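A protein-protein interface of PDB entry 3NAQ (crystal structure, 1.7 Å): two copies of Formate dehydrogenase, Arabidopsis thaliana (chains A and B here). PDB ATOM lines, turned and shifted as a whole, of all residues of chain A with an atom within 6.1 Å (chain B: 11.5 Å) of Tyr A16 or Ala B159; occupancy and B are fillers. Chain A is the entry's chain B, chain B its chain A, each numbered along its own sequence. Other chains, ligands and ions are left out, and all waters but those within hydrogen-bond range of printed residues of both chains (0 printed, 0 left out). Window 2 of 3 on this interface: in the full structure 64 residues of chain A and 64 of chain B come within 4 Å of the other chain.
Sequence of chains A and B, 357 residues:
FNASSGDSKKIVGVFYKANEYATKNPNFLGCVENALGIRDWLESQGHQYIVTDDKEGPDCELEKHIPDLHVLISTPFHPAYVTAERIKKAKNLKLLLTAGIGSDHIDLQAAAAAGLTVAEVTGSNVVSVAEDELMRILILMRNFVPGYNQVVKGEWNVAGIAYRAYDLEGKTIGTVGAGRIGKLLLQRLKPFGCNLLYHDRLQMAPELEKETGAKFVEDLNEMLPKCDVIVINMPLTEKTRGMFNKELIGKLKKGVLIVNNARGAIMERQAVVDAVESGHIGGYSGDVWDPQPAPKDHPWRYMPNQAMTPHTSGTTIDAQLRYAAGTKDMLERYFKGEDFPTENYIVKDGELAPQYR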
ATOM      1  N   VAL A  14       7.481   4.849 -12.954  1.00  0.00           N
ATOM      2  CA  VAL A  14       6.796   4.186 -11.874  1.00  0.00           C
ATOM      3  C   VAL A  14       6.173   2.936 -12.446  1.00  0.00           C
ATOM      4  O   VAL A  14       5.378   3.002 -13.378  1.00  0.00           O
ATOM      5  CB  VAL A  14       5.768   5.048 -11.246  1.00  0.00           C
ATOM      6  CG1 VAL A  14       4.890   4.282 -10.271  1.00  0.00           C
ATOM      7  CG2 VAL A  14       6.447   6.248 -10.559  1.00  0.00           C
ATOM      8  N   PHE A  15       6.573   1.819 -11.875  1.00  0.00           N
ATOM      9  CA  PHE A  15       6.169   0.519 -12.313  1.00  0.00           C
ATOM     10  C   PHE A  15       6.054  -0.397 -11.097  1.00  0.00           C
ATOM     11  O   PHE A  15       6.607  -0.114 -10.021  1.00  0.00           O
ATOM     12  CB  PHE A  15       7.230  -0.096 -13.211  1.00  0.00           C
ATOM     13  CG  PHE A  15       7.697   0.783 -14.330  1.00  0.00           C
ATOM     14  CD1 PHE A  15       8.937   1.380 -14.271  1.00  0.00           C
ATOM     15  CD2 PHE A  15       6.883   1.048 -15.397  1.00  0.00           C
ATOM     16  CE1 PHE A  15       9.390   2.186 -15.276  1.00  0.00           C
ATOM     17  CE2 PHE A  15       7.337   1.878 -16.452  1.00  0.00           C
ATOM     18  CZ  PHE A  15       8.585   2.447 -16.361  1.00  0.00           C
ATOM     19  N   TYR A  16       5.339  -1.500 -11.241  1.00  0.00           N
ATOM     20  CA  TYR A  16       5.366  -2.432 -10.102  1.00  0.00           C
ATOM     21  C   TYR A  16       6.643  -3.208 -10.096  1.00  0.00           C
ATOM     22  O   TYR A  16       7.373  -3.244 -11.083  1.00  0.00           O
ATOM     23  CB  TYR A  16       4.157  -3.335  -9.991  1.00  0.00           C
ATOM     24  CG  TYR A  16       3.879  -4.171 -11.215  1.00  0.00           C
ATOM     25  CD1 TYR A  16       4.683  -5.247 -11.533  1.00  0.00           C
ATOM     26  CD2 TYR A  16       2.751  -3.944 -11.992  1.00  0.00           C
ATOM     27  CE1 TYR A  16       4.416  -6.024 -12.633  1.00  0.00           C
ATOM     28  CE2 TYR A  16       2.456  -4.721 -13.079  1.00  0.00           C
ATOM     29  CZ  TYR A  16       3.294  -5.764 -13.397  1.00  0.00           C
ATOM     30  OH  TYR A  16       3.040  -6.558 -14.486  1.00  0.00           O
ATOM     31  N   LYS A  17       6.941  -3.748  -8.923  1.00  0.00           N
ATOM     32  CA  LYS A  17       8.033  -4.676  -8.768  1.00  0.00           C
ATOM     33  C   LYS A  17       7.518  -6.022  -9.239  1.00  0.00           C
ATOM     34  O   LYS A  17       6.477  -6.524  -8.768  1.00  0.00           O
ATOM     35  CB  LYS A  17       8.462  -4.753  -7.293  1.00  0.00           C
ATOM     36  CG  LYS A  17       9.332  -3.610  -6.913  1.00  0.00           C
ATOM     37  CD  LYS A  17       9.799  -3.676  -5.455  1.00  0.00           C
ATOM     38  CE  LYS A  17      10.974  -4.605  -5.259  1.00  0.00           C
ATOM     39  NZ  LYS A  17      12.066  -3.928  -4.461  1.00  0.00           N
ATOM     40  N   ALA A  18       8.250  -6.600 -10.190  1.00  0.00           N
ATOM     41  CA  ALA A  18       8.022  -7.947 -10.678  1.00  0.00           C
ATOM     42  C   ALA A  18       8.838  -9.008  -9.907  1.00  0.00           C
ATOM     43  O   ALA A  18       8.548 -10.192 -10.037  1.00  0.00           O
ATOM     44  CB  ALA A  18       8.372  -8.010 -12.153  1.00  0.00           C
ATOM     45  N   TYR A  21       9.921 -12.535 -11.233  1.00  0.00           N
ATOM     46  CA  TYR A  21       9.411 -12.605 -12.596  1.00  0.00           C
ATOM     47  C   TYR A  21      10.269 -11.803 -13.559  1.00  0.00           C
ATOM     48  O   TYR A  21      10.341 -12.146 -14.743  1.00  0.00           O
ATOM     49  CB  TYR A  21       7.948 -12.157 -12.616  1.00  0.00           C
ATOM     50  CG  TYR A  21       7.071 -13.007 -11.665  1.00  0.00           C
ATOM     51  CD1 TYR A  21       6.312 -12.413 -10.659  1.00  0.00           C
ATOM     52  CD2 TYR A  21       6.980 -14.370 -11.826  1.00  0.00           C
ATOM     53  CE1 TYR A  21       5.492 -13.185  -9.820  1.00  0.00           C
ATOM     54  CE2 TYR A  21       6.153 -15.153 -10.974  1.00  0.00           C
ATOM     55  CZ  TYR A  21       5.429 -14.522  -9.977  1.00  0.00           C
ATOM     56  OH  TYR A  21       4.625 -15.271  -9.138  1.00  0.00           O
ATOM     57  N   PHE A  28      10.283  -8.831 -19.739  1.00  0.00           N
ATOM     58  CA  PHE A  28       9.175  -8.267 -18.973  1.00  0.00           C
ATOM     59  C   PHE A  28       9.517  -6.807 -18.637  1.00  0.00           C
ATOM     60  O   PHE A  28       9.987  -6.498 -17.542  1.00  0.00           O
ATOM     61  CB  PHE A  28       8.994  -9.115 -17.735  1.00  0.00           C
ATOM     62  CG  PHE A  28       7.790  -8.755 -16.856  1.00  0.00           C
ATOM     63  CD1 PHE A  28       7.436  -9.667 -15.881  1.00  0.00           C
ATOM     64  CD2 PHE A  28       7.036  -7.620 -16.996  1.00  0.00           C
ATOM     65  CE1 PHE A  28       6.352  -9.458 -15.055  1.00  0.00           C
ATOM     66  CE2 PHE A  28       5.937  -7.368 -16.118  1.00  0.00           C
ATOM     67  CZ  PHE A  28       5.612  -8.296 -15.161  1.00  0.00           C
ATOM     68  N   GLY A  30       7.733  -4.026 -18.368  1.00  0.00           N
ATOM     69  CA  GLY A  30       6.824  -3.143 -17.615  1.00  0.00           C
ATOM     70  C   GLY A  30       6.915  -3.351 -16.110  1.00  0.00           C
ATOM     71  O   GLY A  30       5.899  -3.596 -15.446  1.00  0.00           O
ATOM     72  N   CYS A  31       8.129  -3.290 -15.576  1.00  0.00           N
ATOM     73  CA  CYS A  31       8.346  -3.478 -14.150  1.00  0.00           C
ATOM     74  C   CYS A  31       9.548  -2.657 -13.737  1.00  0.00           C
ATOM     75  O   CYS A  31      10.299  -2.170 -14.565  1.00  0.00           O
ATOM     76  CB  CYS A  31       8.573  -4.952 -13.775  1.00  0.00           C
ATOM     77  SG  CYS A  31       9.978  -5.709 -14.515  1.00  0.00           S
ATOM     78  N   VAL A  32       9.698  -2.468 -12.448  1.00  0.00           N
ATOM     79  CA  VAL A  32      10.822  -1.713 -11.927  1.00  0.00           C
ATOM     80  C   VAL A  32      12.177  -2.233 -12.391  1.00  0.00           C
ATOM     81  O   VAL A  32      13.087  -1.443 -12.715  1.00  0.00           O
ATOM     82  CB  VAL A  32      10.775  -1.708 -10.413  1.00  0.00           C
ATOM     83  CG1 VAL A  32      12.103  -1.306  -9.831  1.00  0.00           C
ATOM     84  CG2 VAL A  32       9.675  -0.770  -9.956  1.00  0.00           C
ATOM     85  N   GLU A  33      12.300  -3.563 -12.404  1.00  0.00           N
ATOM     86  CA  GLU A  33      13.562  -4.219 -12.501  1.00  0.00           C
ATOM     87  C   GLU A  33      14.086  -4.055 -13.899  1.00  0.00           C
ATOM     88  O   GLU A  33      15.280  -3.850 -14.078  1.00  0.00           O
ATOM     89  CB  GLU A  33      13.418  -5.684 -12.154  1.00  0.00           C
ATOM     90  CG  GLU A  33      13.131  -5.894 -10.682  1.00  0.00           C
ATOM     91  CD  GLU A  33      11.649  -5.855 -10.299  1.00  0.00           C
ATOM     92  OE1 GLU A  33      10.789  -5.625 -11.141  1.00  0.00           O
ATOM     93  OE2 GLU A  33      11.335  -6.149  -9.132  1.00  0.00           O
ATOM     94  N   THR A  52      10.831   3.544  -9.659  1.00  0.00           N
ATOM     95  CA  THR A  52      10.338   3.161  -8.331  1.00  0.00           C
ATOM     96  C   THR A  52       8.935   2.575  -8.412  1.00  0.00           C
ATOM     97  O   THR A  52       8.171   2.898  -9.299  1.00  0.00           O
ATOM     98  CB  THR A  52      10.368   4.316  -7.337  1.00  0.00           C
ATOM     99  OG1 THR A  52      10.051   3.826  -6.025  1.00  0.00           O
ATOM    100  CG2 THR A  52       9.389   5.394  -7.713  1.00  0.00           C
ATOM    101  N   ASP A  53       8.616   1.677  -7.486  1.00  0.00           N
ATOM    102  CA  ASP A  53       7.220   1.260  -7.304  1.00  0.00           C
ATOM    103  C   ASP A  53       6.523   1.980  -6.180  1.00  0.00           C
ATOM    104  O   ASP A  53       5.338   1.772  -5.973  1.00  0.00           O
ATOM    105  CB  ASP A  53       7.128  -0.230  -7.023  1.00  0.00           C
ATOM    106  CG  ASP A  53       7.592  -0.597  -5.629  1.00  0.00           C
ATOM    107  OD1 ASP A  53       8.600  -0.040  -5.134  1.00  0.00           O
ATOM    108  OD2 ASP A  53       6.936  -1.468  -5.032  1.00  0.00           O
ATOM    109  N   THR A  75       2.457   2.996 -16.116  1.00  0.00           N
ATOM    110  CA  THR A  75       1.586   2.150 -16.889  1.00  0.00           C
ATOM    111  C   THR A  75       0.308   2.092 -16.130  1.00  0.00           C
ATOM    112  O   THR A  75       0.294   2.336 -14.922  1.00  0.00           O
ATOM    113  CB  THR A  75       2.139   0.702 -16.941  1.00  0.00           C
ATOM    114  OG1 THR A  75       1.997   0.126 -15.633  1.00  0.00           O
ATOM    115  CG2 THR A  75       3.574   0.661 -17.362  1.00  0.00           C
ATOM    116  N   PHE A  77      -1.024  -0.423 -14.977  1.00  0.00           N
ATOM    117  CA  PHE A  77      -0.934  -1.533 -14.009  1.00  0.00           C
ATOM    118  C   PHE A  77      -0.446  -1.213 -12.600  1.00  0.00           C
ATOM    119  O   PHE A  77      -0.684  -1.997 -11.658  1.00  0.00           O
ATOM    120  CB  PHE A  77      -0.157  -2.674 -14.628  1.00  0.00           C
ATOM    121  CG  PHE A  77      -0.827  -3.197 -15.815  1.00  0.00           C
ATOM    122  CD1 PHE A  77      -1.816  -4.172 -15.694  1.00  0.00           C
ATOM    123  CD2 PHE A  77      -0.579  -2.629 -17.073  1.00  0.00           C
ATOM    124  CE1 PHE A  77      -2.515  -4.621 -16.819  1.00  0.00           C
ATOM    125  CE2 PHE A  77      -1.265  -3.067 -18.215  1.00  0.00           C
ATOM    126  CZ  PHE A  77      -2.235  -4.069 -18.091  1.00  0.00           C
ATOM    127  N   HIS A  78       0.227  -0.083 -12.452  1.00  0.00           N
ATOM    128  CA  HIS A  78       0.712   0.396 -11.159  1.00  0.00           C
ATOM    129  C   HIS A  78       0.915   1.864 -11.427  1.00  0.00           C
ATOM    130  O   HIS A  78       2.025   2.376 -11.472  1.00  0.00           O
ATOM    131  CB  HIS A  78       2.040  -0.294 -10.823  1.00  0.00           C
ATOM    132  CG  HIS A  78       2.526  -0.046  -9.421  1.00  0.00           C
ATOM    133  ND1 HIS A  78       1.967  -0.655  -8.321  1.00  0.00           N
ATOM    134  CD2 HIS A  78       3.551   0.708  -8.948  1.00  0.00           C
ATOM    135  CE1 HIS A  78       2.612  -0.281  -7.225  1.00  0.00           C
ATOM    136  NE2 HIS A  78       3.578   0.547  -7.580  1.00  0.00           N
ATOM    137  N   THR A 315      -1.058  -6.762 -21.503  1.00  0.00           N
ATOM    138  CA  THR A 315       0.268  -6.672 -20.898  1.00  0.00           C
ATOM    139  C   THR A 315       1.033  -7.974 -21.128  1.00  0.00           C
ATOM    140  O   THR A 315       1.887  -8.458 -20.338  1.00  0.00           O
ATOM    141  CB  THR A 315       0.183  -6.198 -19.430  1.00  0.00           C
ATOM    142  OG1 THR A 315       1.502  -5.796 -19.003  1.00  0.00           O
ATOM    143  CG2 THR A 315      -0.351  -7.265 -18.568  1.00  0.00           C
ATOM    144  N   GLN A 320       3.975  -5.230 -24.139  1.00  0.00           N
ATOM    145  CA  GLN A 320       4.952  -4.485 -23.339  1.00  0.00           C
ATOM    146  C   GLN A 320       6.091  -3.998 -24.217  1.00  0.00           C
ATOM    147  O   GLN A 320       6.568  -2.884 -24.030  1.00  0.00           O
ATOM    148  CB  GLN A 320       5.474  -5.344 -22.210  1.00  0.00           C
ATOM    149  CG  GLN A 320       4.434  -5.628 -21.072  1.00  0.00           C
ATOM    150  CD  GLN A 320       5.051  -6.336 -19.885  1.00  0.00           C
ATOM    151  OE1 GLN A 320       6.185  -6.006 -19.476  1.00  0.00           O
ATOM    152  NE2 GLN A 320       4.390  -7.375 -19.383  1.00  0.00           N
ATOM    153  N   ARG B 142      -0.862 -17.309 -24.480  1.00  0.00           N
ATOM    154  CA  ARG B 142      -1.399 -16.148 -23.747  1.00  0.00           C
ATOM    155  C   ARG B 142      -1.505 -16.393 -22.250  1.00  0.00           C
ATOM    156  O   ARG B 142      -1.886 -15.500 -21.497  1.00  0.00           O
ATOM    157  CB  ARG B 142      -2.731 -15.729 -24.360  1.00  0.00           C
ATOM    158  CG  ARG B 142      -2.672 -15.411 -25.820  1.00  0.00           C
ATOM    159  CD  ARG B 142      -3.909 -14.687 -26.381  1.00  0.00           C
ATOM    160  NE  ARG B 142      -4.117 -13.483 -25.603  1.00  0.00           N
ATOM    161  CZ  ARG B 142      -3.416 -12.354 -25.727  1.00  0.00           C
ATOM    162  NH1 ARG B 142      -2.567 -12.184 -26.718  1.00  0.00           N
ATOM    163  NH2 ARG B 142      -3.589 -11.389 -24.842  1.00  0.00           N
ATOM    164  N   ASN B 143      -1.155 -17.600 -21.812  1.00  0.00           N
ATOM    165  CA  ASN B 143      -1.040 -17.940 -20.391  1.00  0.00           C
ATOM    166  C   ASN B 143      -2.353 -17.794 -19.622  1.00  0.00           C
ATOM    167  O   ASN B 143      -2.382 -17.210 -18.551  1.00  0.00           O
ATOM    168  CB  ASN B 143       0.045 -17.072 -19.741  1.00  0.00           C
ATOM    169  CG  ASN B 143       0.738 -17.774 -18.626  1.00  0.00           C
ATOM    170  OD1 ASN B 143       0.888 -19.005 -18.669  1.00  0.00           O
ATOM    171  ND2 ASN B 143       1.179 -17.021 -17.632  1.00  0.00           N
ATOM    172  N   PRO B 146      -2.812 -19.890 -15.568  1.00  0.00           N
ATOM    173  CA  PRO B 146      -2.437 -19.227 -14.306  1.00  0.00           C
ATOM    174  C   PRO B 146      -3.351 -18.069 -13.979  1.00  0.00           C
ATOM    175  O   PRO B 146      -3.682 -17.851 -12.844  1.00  0.00           O
ATOM    176  CB  PRO B 146      -1.024 -18.702 -14.584  1.00  0.00           C
ATOM    177  CG  PRO B 146      -0.509 -19.569 -15.667  1.00  0.00           C
ATOM    178  CD  PRO B 146      -1.687 -19.949 -16.500  1.00  0.00           C
ATOM    179  N   GLY B 147      -3.794 -17.340 -14.989  1.00  0.00           N
ATOM    180  CA  GLY B 147      -4.791 -16.298 -14.784  1.00  0.00           C
ATOM    181  C   GLY B 147      -6.094 -16.838 -14.257  1.00  0.00           C
ATOM    182  O   GLY B 147      -6.629 -16.307 -13.304  1.00  0.00           O
ATOM    183  N   GLN B 150      -5.749 -17.878 -10.508  1.00  0.00           N
ATOM    184  CA  GLN B 150      -5.759 -16.750  -9.565  1.00  0.00           C
ATOM    185  C   GLN B 150      -7.178 -16.306  -9.256  1.00  0.00           C
ATOM    186  O   GLN B 150      -7.466 -15.862  -8.154  1.00  0.00           O
ATOM    187  CB  GLN B 150      -5.018 -15.560 -10.173  1.00  0.00           C
ATOM    188  CG  GLN B 150      -3.525 -15.640 -10.055  1.00  0.00           C
ATOM    189  CD  GLN B 150      -2.837 -14.361 -10.481  1.00  0.00           C
ATOM    190  OE1 GLN B 150      -3.436 -13.305 -10.487  1.00  0.00           O
ATOM    191  NE2 GLN B 150      -1.550 -14.452 -10.787  1.00  0.00           N
ATOM    192  N   GLU B 155      -6.848 -14.345  -5.839  1.00  0.00           N
ATOM    193  CA  GLU B 155      -5.615 -13.624  -6.091  1.00  0.00           C
ATOM    194  C   GLU B 155      -5.779 -12.557  -7.180  1.00  0.00           C
ATOM    195  O   GLU B 155      -6.790 -12.513  -7.917  1.00  0.00           O
ATOM    196  CB  GLU B 155      -4.511 -14.628  -6.436  1.00  0.00           C
ATOM    197  CG  GLU B 155      -4.157 -15.572  -5.280  1.00  0.00           C
ATOM    198  CD  GLU B 155      -3.261 -16.736  -5.692  1.00  0.00           C
ATOM    199  OE1 GLU B 155      -2.859 -16.795  -6.861  1.00  0.00           O
ATOM    200  OE2 GLU B 155      -2.957 -17.600  -4.840  1.00  0.00           O
ATOM    201  N   TRP B 156      -4.771 -11.694  -7.266  1.00  0.00           N
ATOM    202  CA  TRP B 156      -4.658 -10.687  -8.306  1.00  0.00           C
ATOM    203  C   TRP B 156      -3.193 -10.278  -8.370  1.00  0.00           C
ATOM    204  O   TRP B 156      -2.743  -9.401  -7.632  1.00  0.00           O
ATOM    205  CB  TRP B 156      -5.541  -9.466  -8.048  1.00  0.00           C
ATOM    206  CG  TRP B 156      -5.578  -8.496  -9.235  1.00  0.00           C
ATOM    207  CD1 TRP B 156      -4.621  -7.598  -9.589  1.00  0.00           C
ATOM    208  CD2 TRP B 156      -6.622  -8.370 -10.221  1.00  0.00           C
ATOM    209  NE1 TRP B 156      -5.007  -6.899 -10.710  1.00  0.00           N
ATOM    210  CE2 TRP B 156      -6.241  -7.340 -11.104  1.00  0.00           C
ATOM    211  CE3 TRP B 156      -7.860  -8.971 -10.391  1.00  0.00           C
ATOM    212  CZ2 TRP B 156      -7.042  -6.920 -12.148  1.00  0.00           C
ATOM    213  CZ3 TRP B 156      -8.655  -8.568 -11.451  1.00  0.00           C
ATOM    214  CH2 TRP B 156      -8.237  -7.559 -12.325  1.00  0.00           C
ATOM    215  N   ASN B 157      -2.473 -10.972  -9.246  1.00  0.00           N
ATOM    216  CA  ASN B 157      -1.039 -10.858  -9.392  1.00  0.00           C
ATOM    217  C   ASN B 157      -0.721 -10.848 -10.888  1.00  0.00           C
ATOM    218  O   ASN B 157      -0.432 -11.876 -11.482  1.00  0.00           O
ATOM    219  CB  ASN B 157      -0.428 -12.066  -8.675  1.00  0.00           C
ATOM    220  CG  ASN B 157       1.061 -12.180  -8.857  1.00  0.00           C
ATOM    221  OD1 ASN B 157       1.741 -11.216  -9.222  1.00  0.00           O
ATOM    222  ND2 ASN B 157       1.589 -13.375  -8.578  1.00  0.00           N
ATOM    223  N   VAL B 158      -0.819  -9.671 -11.497  1.00  0.00           N
ATOM    224  CA  VAL B 158      -0.638  -9.538 -12.922  1.00  0.00           C
ATOM    225  C   VAL B 158       0.756 -10.024 -13.303  1.00  0.00           C
ATOM    226  O   VAL B 158       0.896 -10.724 -14.283  1.00  0.00           O
ATOM    227  CB  VAL B 158      -0.849  -8.087 -13.373  1.00  0.00           C
ATOM    228  CG1 VAL B 158      -0.536  -7.916 -14.874  1.00  0.00           C
ATOM    229  CG2 VAL B 158      -2.316  -7.649 -13.054  1.00  0.00           C
ATOM    230  N   ALA B 159       1.764  -9.683 -12.505  1.00  0.00           N
ATOM    231  CA  ALA B 159       3.150 -10.000 -12.875  1.00  0.00           C
ATOM    232  C   ALA B 159       3.338 -11.491 -13.066  1.00  0.00           C
ATOM    233  O   ALA B 159       4.022 -11.952 -14.015  1.00  0.00           O
ATOM    234  CB  ALA B 159       4.130  -9.465 -11.844  1.00  0.00           C
ATOM    235  N   GLY B 160       2.696 -12.244 -12.175  1.00  0.00           N
ATOM    236  CA  GLY B 160       2.745 -13.687 -12.174  1.00  0.00           C
ATOM    237  C   GLY B 160       2.203 -14.350 -13.397  1.00  0.00           C
ATOM    238  O   GLY B 160       2.470 -15.507 -13.614  1.00  0.00           O
ATOM    239  N   ILE B 161       1.390 -13.618 -14.154  1.00  0.00           N
ATOM    240  CA  ILE B 161       0.784 -14.078 -15.386  1.00  0.00           C
ATOM    241  C   ILE B 161       1.512 -13.471 -16.553  1.00  0.00           C
ATOM    242  O   ILE B 161       1.826 -14.187 -17.482  1.00  0.00           O
ATOM    243  CB  ILE B 161      -0.677 -13.650 -15.501  1.00  0.00           C
ATOM    244  CG1 ILE B 161      -1.482 -14.250 -14.354  1.00  0.00           C
ATOM    245  CG2 ILE B 161      -1.279 -14.110 -16.835  1.00  0.00           C
ATOM    246  CD1 ILE B 161      -2.640 -13.386 -13.983  1.00  0.00           C
ATOM    247  N   ALA B 162       1.769 -12.162 -16.491  1.00  0.00           N
ATOM    248  CA  ALA B 162       2.362 -11.426 -17.635  1.00  0.00           C
ATOM    249  C   ALA B 162       3.734 -11.976 -18.061  1.00  0.00           C
ATOM    250  O   ALA B 162       4.077 -11.991 -19.229  1.00  0.00           O
ATOM    251  CB  ALA B 162       2.471  -9.950 -17.312  1.00  0.00           C
ATOM    252  N   TYR B 163       4.513 -12.473 -17.099  1.00  0.00           N
ATOM    253  CA  TYR B 163       5.907 -12.820 -17.396  1.00  0.00           C
ATOM    254  C   TYR B 163       6.014 -13.995 -18.353  1.00  0.00           C
ATOM    255  O   TYR B 163       7.079 -14.202 -18.961  1.00  0.00           O
ATOM    256  CB  TYR B 163       6.680 -13.080 -16.107  1.00  0.00           C
ATOM    257  CG  TYR B 163       6.671 -14.500 -15.564  1.00  0.00           C
ATOM    258  CD1 TYR B 163       7.814 -15.289 -15.611  1.00  0.00           C
ATOM    259  CD2 TYR B 163       5.546 -15.019 -14.939  1.00  0.00           C
ATOM    260  CE1 TYR B 163       7.833 -16.592 -15.070  1.00  0.00           C
ATOM    261  CE2 TYR B 163       5.540 -16.319 -14.422  1.00  0.00           C
ATOM    262  CZ  TYR B 163       6.679 -17.100 -14.474  1.00  0.00           C
ATOM    263  OH  TYR B 163       6.658 -18.384 -13.934  1.00  0.00           O
ATOM    264  N   ARG B 164       4.927 -14.763 -18.501  1.00  0.00           N
ATOM    265  CA  ARG B 164       4.904 -15.873 -19.433  1.00  0.00           C
ATOM    266  C   ARG B 164       3.776 -15.755 -20.443  1.00  0.00           C
ATOM    267  O   ARG B 164       3.366 -16.767 -21.013  1.00  0.00           O
ATOM    268  CB  ARG B 164       4.803 -17.213 -18.660  1.00  0.00           C
ATOM    269  CG  ARG B 164       6.002 -17.519 -17.808  1.00  0.00           C
ATOM    270  CD  ARG B 164       7.292 -17.702 -18.658  1.00  0.00           C
ATOM    271  NE  ARG B 164       8.429 -18.189 -17.850  1.00  0.00           N
ATOM    272  CZ  ARG B 164       9.701 -17.800 -17.980  1.00  0.00           C
ATOM    273  NH1 ARG B 164      10.068 -16.900 -18.896  1.00  0.00           N
ATOM    274  NH2 ARG B 164      10.626 -18.320 -17.170  1.00  0.00           N
ATOM    275  N   ALA B 165       3.239 -14.543 -20.622  1.00  0.00           N
ATOM    276  CA  ALA B 165       2.136 -14.325 -21.538  1.00  0.00           C
ATOM    277  C   ALA B 165       2.625 -13.547 -22.771  1.00  0.00           C
ATOM    278  O   ALA B 165       3.296 -12.526 -22.637  1.00  0.00           O
ATOM    279  CB  ALA B 165       1.046 -13.565 -20.834  1.00  0.00           C
ATOM    280  N   TYR B 166       2.306 -14.064 -23.948  1.00  0.00           N
ATOM    281  CA  TYR B 166       2.737 -13.504 -25.209  1.00  0.00           C
ATOM    282  C   TYR B 166       1.575 -13.450 -26.125  1.00  0.00           C
ATOM    283  O   TYR B 166       0.646 -14.198 -25.956  1.00  0.00           O
ATOM    284  CB  TYR B 166       3.775 -14.426 -25.832  1.00  0.00           C
ATOM    285  CG  TYR B 166       5.117 -14.332 -25.134  1.00  0.00           C
ATOM    286  CD1 TYR B 166       6.108 -13.555 -25.652  1.00  0.00           C
ATOM    287  CD2 TYR B 166       5.388 -15.033 -23.951  1.00  0.00           C
ATOM    288  CE1 TYR B 166       7.353 -13.435 -25.049  1.00  0.00           C
ATOM    289  CE2 TYR B 166       6.623 -14.903 -23.344  1.00  0.00           C
ATOM    290  CZ  TYR B 166       7.610 -14.132 -23.920  1.00  0.00           C
ATOM    291  OH  TYR B 166       8.877 -13.944 -23.372  1.00  0.00           O
ATOM    292  N   ASN B 305       2.565 -25.962 -15.411  1.00  0.00           N
ATOM    293  CA  ASN B 305       2.182 -25.370 -16.662  1.00  0.00           C
ATOM    294  C   ASN B 305       1.341 -26.243 -17.600  1.00  0.00           C
ATOM    295  O   ASN B 305       1.154 -25.873 -18.776  1.00  0.00           O
ATOM    296  CB  ASN B 305       3.433 -24.891 -17.373  1.00  0.00           C
ATOM    297  CG  ASN B 305       4.162 -23.857 -16.589  1.00  0.00           C
ATOM    298  OD1 ASN B 305       3.547 -22.909 -16.084  1.00  0.00           O
ATOM    299  ND2 ASN B 305       5.472 -23.988 -16.509  1.00  0.00           N
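The backbone carbonyl oxygen (O) of Phe A28 lies within hydrogen-bond range of the side-chain sulfur (SG) of Cys A31, at 3.1 Å. The side-chain amide nitrogen of Gln A320 lies within hydrogen-bond range of the backbone carbonyl oxygen of Thr A315 (2.9 Å). OD1 of Asn B157 is in hydrogen-bond range of N of Gly B160, at 3.3 Å. The side-chain amide oxygen (OE1) of Gln A320 lies within hydrogen-bond range of the backbone NH (N) of Gly A30, 2.7 Å away. The side-chain amide oxygen (OE1) of Gln B150 is in hydrogen-bond range of the backbone NH (N) of Asn B157 (2.8 Å). O of Tyr A16 is in hydrogen-bond range of N of Val A32 (2.8 Å).
Among the printed residues, pairs that only touch across the chains: Thr A315 with Ala B162, Tyr A21 with Tyr B163, Phe A28 with Tyr B163, Tyr A16 with Ala B159, Tyr A21 with Gly B160, Phe A28 with Ala B159, Tyr A21 with Asn B157, Thr A315 with Val B158, Gln A320 with Ala B162, Tyr A16 with Val B158 and Tyr A21 with Ala B159.
No residue of chain B comes within 4 Å of Phe A15. Tyr A16 touches just these residues of chain B: Val B158 (3.8 Å) and Ala B159 (3.5 Å). Ala A18 touches none of the printed residues of chain B. Of the printed residues of chain B, Tyr A21 touches Asn B157 (3.6 Å), Ala B159 (3.9 Å), Gly B160 (3.6 Å) and Tyr B163 (3.5 Å). Of the printed residues of chain B, Phe A28 touches Ala B159 (3.6 Å) and Tyr B163 (3.5 Å). Gly A30 touches none of the printed residues of chain B. No residue of chain B comes within 4 Å of Cys A31. No residue of chain B comes within 4 Å of Val A32. No residue of chain B comes within 4 Å of Asp A53. No residue of chain B comes within 4 Å of Phe A77. No residue of chain B comes within 4 Å of His A78. Of the printed residues of chain A, Asn B157 touches Tyr A21. Ala B159 touches just these residues of chain A: Tyr A16, Tyr A21 and Phe A28. Of the printed residues of chain A, Ala B162 touches Thr A315 (3.4 Å) and Gln A320 (3.8 Å). The nearest residue of chain B that does not touch Tyr A16 is Ala B162 (4.5 Å). The nearest residue of chain A that does not touch Ala B159 is Ala A18 (4.3 Å). The nearest printed residue of chain A that does not touch Ala B162 is Phe A28 (4.2 Å).
Hydrophobic or aromatic side chains of chain A that line the printed part of chain B: Tyr A16, Tyr A21 and Phe A28. Among the printed residues, no Asp or Glu carboxylate lies within 4 Å of a Lys or Arg side-chain nitrogen of the other chain.
No position is printed for both chains.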
